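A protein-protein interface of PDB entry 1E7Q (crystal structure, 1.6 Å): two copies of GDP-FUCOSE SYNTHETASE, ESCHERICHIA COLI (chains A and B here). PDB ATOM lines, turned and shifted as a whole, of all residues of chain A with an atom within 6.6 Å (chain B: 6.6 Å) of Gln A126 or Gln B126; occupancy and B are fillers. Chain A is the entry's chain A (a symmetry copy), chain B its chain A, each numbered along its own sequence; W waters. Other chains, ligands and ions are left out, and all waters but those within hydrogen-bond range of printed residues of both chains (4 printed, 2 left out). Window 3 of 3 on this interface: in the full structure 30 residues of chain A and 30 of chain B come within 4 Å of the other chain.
Among the printed residues, pairs that only touch across the chains: Leu A124 with Thr B128, Gln A126 with Gly B127, Gln A126 with Thr B128, Gly A127 with Gln B126, Thr A128 with Leu B124 and Thr A128 with Gln B126.
Of the 9 printed residues of chain A, 5 touch a printed residue of chain B. Printed residues of chain A that touch a printed residue of chain B: Leu A124, Leu A125, Gln A126, Gly A127 and Thr A128. Among the printed residues, 11 pairs touch across the chains. Among the printed residues, no Asp or Glu carboxylate lies within 4 Å of a Lys or Arg side-chain nitrogen of the other chain.
Water W1 lies within hydrogen-bond range of NE2 of Gln A126 (2.5 Å) and N of Thr B128 (2.9 Å). Water W3 lies within hydrogen-bond range of the side-chain amide nitrogen (NE2) of Gln B126 (2.5 Å) and the backbone NH (N) of Thr A128 (2.9 Å). Water W4 lies within hydrogen-bond range of the backbone carbonyl oxygen of Gln B126 and the backbone carbonyl oxygen of Gln A126. Water W2 bridges the backbone carbonyl oxygen of Gln A126 (3.0 Å) and the backbone carbonyl oxygen of Gln B126 (3.0 Å).
Leu A125 touches Gly B127, and with the chains exchanged Gly A127 touches Leu B125. Leu A125 touches Thr B128, and with the chains exchanged Thr A128 touches Leu B125. Gln A126 touches Gly B127, and with the chains exchanged Gly A127 touches Gln B126. Gln A126 touches Thr B128, and with the chains exchanged Thr A128 touches Gln B126. Positions printed for both chains: 112, 115, 122, 123, 124, 125, 126, 127 and 128. Of the 11 pairs that touch across the chains among the printed residues, 11 have their exchanged pair printed and touching as well.
The backbone carbonyl oxygen of Ser B122 lies close to the side-chain amide oxygen of Gln B126 (2.9 Å). The backbone carbonyl oxygen (O) of Ser A122 sits close to the side-chain amide oxygen (OE1) of Gln A126, at 2.9 Å.
O of Gln A126 lies close to O of Gln B126 (3.1 Å). The backbone carbonyl oxygen of Leu A125 lies within hydrogen-bond range of the backbone NH of Thr B128. The backbone carbonyl oxygen (O) of Gly B127 lies close to the backbone carbonyl oxygen (O) of Leu A125 (3.2 Å). The backbone carbonyl oxygen (O) of Gly A127 lies close to the backbone carbonyl oxygen (O) of Leu B125 (3.2 Å). O of Leu B125 is in hydrogen-bond range of N of Thr A128 (3.4 Å).
Gln A126 touches three residues of chain B. Of chain A, only Gln A126 (3.1 Å), Gly A127 (3.7 Å) and Thr A128 (3.6 Å) come within 4 Å of Gln B126. Printed residues of chain A within 4 Å of Gly B127: Leu A125 and Gln A126. Printed residues of chain B within 4 Å of Leu A124: Thr B128 (3.9 Å). Printed residues of chain B within 4 Å of Thr A128: Leu B124 (3.9 Å), Leu B125 (3.4 Å) and Gln B126 (3.6 Å). Ala A115 touches none of the printed residues of chain B. Ala B115 touches none of the printed residues of chain A. The nearest residue of chain B that does not touch Gln A126 is Leu B125 (4.8 Å).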
ATOM      1  N   PRO A 112      13.933  27.330  25.140  1.00  0.00           N
ATOM      2  CA  PRO A 112      13.218  26.918  26.358  1.00  0.00           C
ATOM      3  C   PRO A 112      13.981  25.886  27.156  1.00  0.00           C
ATOM      4  O   PRO A 112      14.667  25.045  26.581  1.00  0.00           O
ATOM      5  CB  PRO A 112      11.898  26.372  25.781  1.00  0.00           C
ATOM      6  CG  PRO A 112      11.772  27.102  24.480  1.00  0.00           C
ATOM      7  CD  PRO A 112      13.164  27.128  23.880  1.00  0.00           C
ATOM      8  N   ALA A 115      13.036  22.371  26.001  1.00  0.00           N
ATOM      9  CA  ALA A 115      13.025  22.198  24.555  1.00  0.00           C
ATOM     10  C   ALA A 115      13.201  20.741  24.159  1.00  0.00           C
ATOM     11  O   ALA A 115      14.020  19.983  24.765  1.00  0.00           O
ATOM     12  CB  ALA A 115      14.126  23.022  23.923  1.00  0.00           C
ATOM     13  N   SER A 122      13.128  26.128  15.308  1.00  0.00           N
ATOM     14  CA  SER A 122      11.730  26.302  15.622  1.00  0.00           C
ATOM     15  C   SER A 122      11.432  26.058  17.105  1.00  0.00           C
ATOM     16  O   SER A 122      10.319  26.370  17.536  1.00  0.00           O
ATOM     17  CB  SER A 122      10.874  25.319  14.784  1.00  0.00           C
ATOM     18  OG  SER A 122      11.294  23.977  15.039  1.00  0.00           O
ATOM     19  N   GLU A 123      12.365  25.565  17.924  1.00  0.00           N
ATOM     20  CA  GLU A 123      12.107  25.493  19.363  1.00  0.00           C
ATOM     21  C   GLU A 123      12.043  26.880  19.997  1.00  0.00           C
ATOM     22  O   GLU A 123      11.609  27.003  21.164  1.00  0.00           O
ATOM     23  CB  GLU A 123      13.204  24.665  20.057  1.00  0.00           C
ATOM     24  CG  GLU A 123      13.203  23.182  19.797  1.00  0.00           C
ATOM     25  CD  GLU A 123      11.965  22.453  20.216  1.00  0.00           C
ATOM     26  OE1 GLU A 123      11.365  22.647  21.296  1.00  0.00           O
ATOM     27  OE2 GLU A 123      11.347  21.770  19.373  1.00  0.00           O
ATOM     28  N   LEU A 124      12.565  27.906  19.311  1.00  0.00           N
ATOM     29  CA  LEU A 124      12.584  29.232  19.939  1.00  0.00           C
ATOM     30  C   LEU A 124      11.167  29.648  20.350  1.00  0.00           C
ATOM     31  O   LEU A 124      10.210  29.497  19.592  1.00  0.00           O
ATOM     32  CB  LEU A 124      13.286  30.261  19.056  1.00  0.00           C
ATOM     33  CG  LEU A 124      13.586  31.628  19.756  1.00  0.00           C
ATOM     34  CD1 LEU A 124      14.695  31.375  20.781  1.00  0.00           C
ATOM     35  CD2 LEU A 124      14.097  32.571  18.646  1.00  0.00           C
ATOM     36  N   LEU A 125      11.048  30.157  21.600  1.00  0.00           N
ATOM     37  CA  LEU A 125       9.767  30.660  22.102  1.00  0.00           C
ATOM     38  C   LEU A 125       8.685  29.617  22.351  1.00  0.00           C
ATOM     39  O   LEU A 125       7.553  29.956  22.709  1.00  0.00           O
ATOM     40  CB  LEU A 125       9.211  31.848  21.283  1.00  0.00           C
ATOM     41  CG  LEU A 125       9.989  33.157  21.467  1.00  0.00           C
ATOM     42  CD1 LEU A 125       9.824  34.138  20.321  1.00  0.00           C
ATOM     43  CD2 LEU A 125       9.682  33.846  22.762  1.00  0.00           C
ATOM     44  N   GLN A 126       9.050  28.320  22.274  1.00  0.00           N
ATOM     45  CA  GLN A 126       8.071  27.272  22.515  1.00  0.00           C
ATOM     46  C   GLN A 126       7.822  26.895  23.970  1.00  0.00           C
ATOM     47  O   GLN A 126       6.856  26.135  24.223  1.00  0.00           O
ATOM     48  CB  GLN A 126       8.385  25.952  21.797  1.00  0.00           C
ATOM     49  CG  GLN A 126       8.553  26.120  20.334  1.00  0.00           C
ATOM     50  CD  GLN A 126       7.372  25.947  19.455  1.00  0.00           C
ATOM     51  OE1 GLN A 126       7.597  25.800  18.244  1.00  0.00           O
ATOM     52  NE2 GLN A 126       6.240  25.704  20.068  1.00  0.00           N
ATOM     53  N   GLY A 127       8.396  27.633  24.906  1.00  0.00           N
ATOM     54  CA  GLY A 127       8.143  27.333  26.316  1.00  0.00           C
ATOM     55  C   GLY A 127       9.025  28.233  27.174  1.00  0.00           C
ATOM     56  O   GLY A 127       9.853  28.982  26.694  1.00  0.00           O
ATOM     57  N   THR A 128       8.906  28.031  28.487  1.00  0.00           N
ATOM     58  CA  THR A 128       9.560  28.948  29.401  1.00  0.00           C
ATOM     59  C   THR A 128      11.058  28.805  29.453  1.00  0.00           C
ATOM     60  O   THR A 128      11.616  27.746  29.151  1.00  0.00           O
ATOM     61  CB  THR A 128       8.841  28.903  30.717  1.00  0.00           C
ATOM     62  OG1 THR A 128       8.991  27.573  31.104  1.00  0.00           O
ATOM     63  CG2 THR A 128       7.416  29.344  30.786  1.00  0.00           C
ATOM     64  N   PRO B 112       0.749  33.384  24.612  1.00  0.00           N
ATOM     65  CA  PRO B 112       0.859  32.484  23.454  1.00  0.00           C
ATOM     66  C   PRO B 112      -0.448  32.337  22.709  1.00  0.00           C
ATOM     67  O   PRO B 112      -1.512  32.357  23.321  1.00  0.00           O
ATOM     68  CB  PRO B 112       1.322  31.172  24.115  1.00  0.00           C
ATOM     69  CG  PRO B 112       2.003  31.645  25.361  1.00  0.00           C
ATOM     70  CD  PRO B 112       1.139  32.764  25.910  1.00  0.00           C
ATOM     71  N   ALA B 115      -2.462  29.433  24.154  1.00  0.00           N
ATOM     72  CA  ALA B 115      -2.537  29.419  25.608  1.00  0.00           C
ATOM     73  C   ALA B 115      -3.744  28.641  26.105  1.00  0.00           C
ATOM     74  O   ALA B 115      -4.873  28.727  25.530  1.00  0.00           O
ATOM     75  CB  ALA B 115      -2.605  30.836  26.139  1.00  0.00           C
ATOM     76  N   SER B 122       0.697  32.726  34.529  1.00  0.00           N
ATOM     77  CA  SER B 122       1.727  31.755  34.250  1.00  0.00           C
ATOM     78  C   SER B 122       1.684  31.261  32.800  1.00  0.00           C
ATOM     79  O   SER B 122       2.630  30.586  32.386  1.00  0.00           O
ATOM     80  CB  SER B 122       1.566  30.532  35.187  1.00  0.00           C
ATOM     81  OG  SER B 122       0.265  29.963  35.019  1.00  0.00           O
ATOM     82  N   GLU B 123       0.675  31.589  31.989  1.00  0.00           N
ATOM     83  CA  GLU B 123       0.739  31.240  30.569  1.00  0.00           C
ATOM     84  C   GLU B 123       1.813  32.041  29.836  1.00  0.00           C
ATOM     85  O   GLU B 123       2.148  31.704  28.679  1.00  0.00           O
ATOM     86  CB  GLU B 123      -0.626  31.485  29.901  1.00  0.00           C
ATOM     87  CG  GLU B 123      -1.742  30.545  30.271  1.00  0.00           C
ATOM     88  CD  GLU B 123      -1.505  29.102  29.950  1.00  0.00           C
ATOM     89  OE1 GLU B 123      -1.005  28.692  28.880  1.00  0.00           O
ATOM     90  OE2 GLU B 123      -1.593  28.254  30.862  1.00  0.00           O
ATOM     91  N   LEU B 124       2.275  33.151  30.426  1.00  0.00           N
ATOM     92  CA  LEU B 124       3.248  33.977  29.701  1.00  0.00           C
ATOM     93  C   LEU B 124       4.471  33.140  29.309  1.00  0.00           C
ATOM     94  O   LEU B 124       5.004  32.372  30.108  1.00  0.00           O
ATOM     95  CB  LEU B 124       3.603  35.241  30.480  1.00  0.00           C
ATOM     96  CG  LEU B 124       4.421  36.300  29.671  1.00  0.00           C
ATOM     97  CD1 LEU B 124       3.474  36.903  28.630  1.00  0.00           C
ATOM     98  CD2 LEU B 124       4.843  37.381  30.689  1.00  0.00           C
ATOM     99  N   LEU B 125       4.892  33.285  28.029  1.00  0.00           N
ATOM    100  CA  LEU B 125       6.089  32.601  27.535  1.00  0.00           C
ATOM    101  C   LEU B 125       5.992  31.087  27.402  1.00  0.00           C
ATOM    102  O   LEU B 125       6.973  30.420  27.058  1.00  0.00           O
ATOM    103  CB  LEU B 125       7.380  33.008  28.282  1.00  0.00           C
ATOM    104  CG  LEU B 125       7.863  34.431  27.975  1.00  0.00           C
ATOM    105  CD1 LEU B 125       8.753  35.026  29.050  1.00  0.00           C
ATOM    106  CD2 LEU B 125       8.540  34.548  26.643  1.00  0.00           C
ATOM    107  N   GLN B 126       4.773  30.530  27.563  1.00  0.00           N
ATOM    108  CA  GLN B 126       4.606  29.092  27.434  1.00  0.00           C
ATOM    109  C   GLN B 126       4.431  28.551  26.020  1.00  0.00           C
ATOM    110  O   GLN B 126       4.474  27.307  25.858  1.00  0.00           O
ATOM    111  CB  GLN B 126       3.424  28.530  28.236  1.00  0.00           C
ATOM    112  CG  GLN B 126       3.492  28.876  29.677  1.00  0.00           C
ATOM    113  CD  GLN B 126       4.159  27.932  30.606  1.00  0.00           C
ATOM    114  OE1 GLN B 126       3.943  28.098  31.816  1.00  0.00           O
ATOM    115  NE2 GLN B 126       4.689  26.869  30.052  1.00  0.00           N
ATOM    116  N   GLY B 127       4.586  29.394  25.012  1.00  0.00           N
ATOM    117  CA  GLY B 127       4.475  28.904  23.638  1.00  0.00           C
ATOM    118  C   GLY B 127       4.555  30.091  22.686  1.00  0.00           C
ATOM    119  O   GLY B 127       4.602  31.240  23.081  1.00  0.00           O
ATOM    120  N   THR B 128       4.434  29.773  21.397  1.00  0.00           N
ATOM    121  CA  THR B 128       4.674  30.794  20.395  1.00  0.00           C
ATOM    122  C   THR B 128       3.590  31.835  20.303  1.00  0.00           C
ATOM    123  O   THR B 128       2.434  31.596  20.663  1.00  0.00           O
ATOM    124  CB  THR B 128       5.062  30.122  19.112  1.00  0.00           C
ATOM    125  OG1 THR B 128       3.942  29.346  18.819  1.00  0.00           O
ATOM    126  CG2 THR B 128       6.320  29.320  19.059  1.00  0.00           C
HETATM  127  O   HOH W   1       4.253  26.858  21.099  1.00  0.00           O
HETATM  128  O   HOH W   2       5.803  24.739  26.618  1.00  0.00           O
HETATM  129  O   HOH W   3       6.821  26.031  29.006  1.00  0.00           O
HETATM  130  O   HOH W   4       4.016  25.427  23.610  1.00  0.00           O
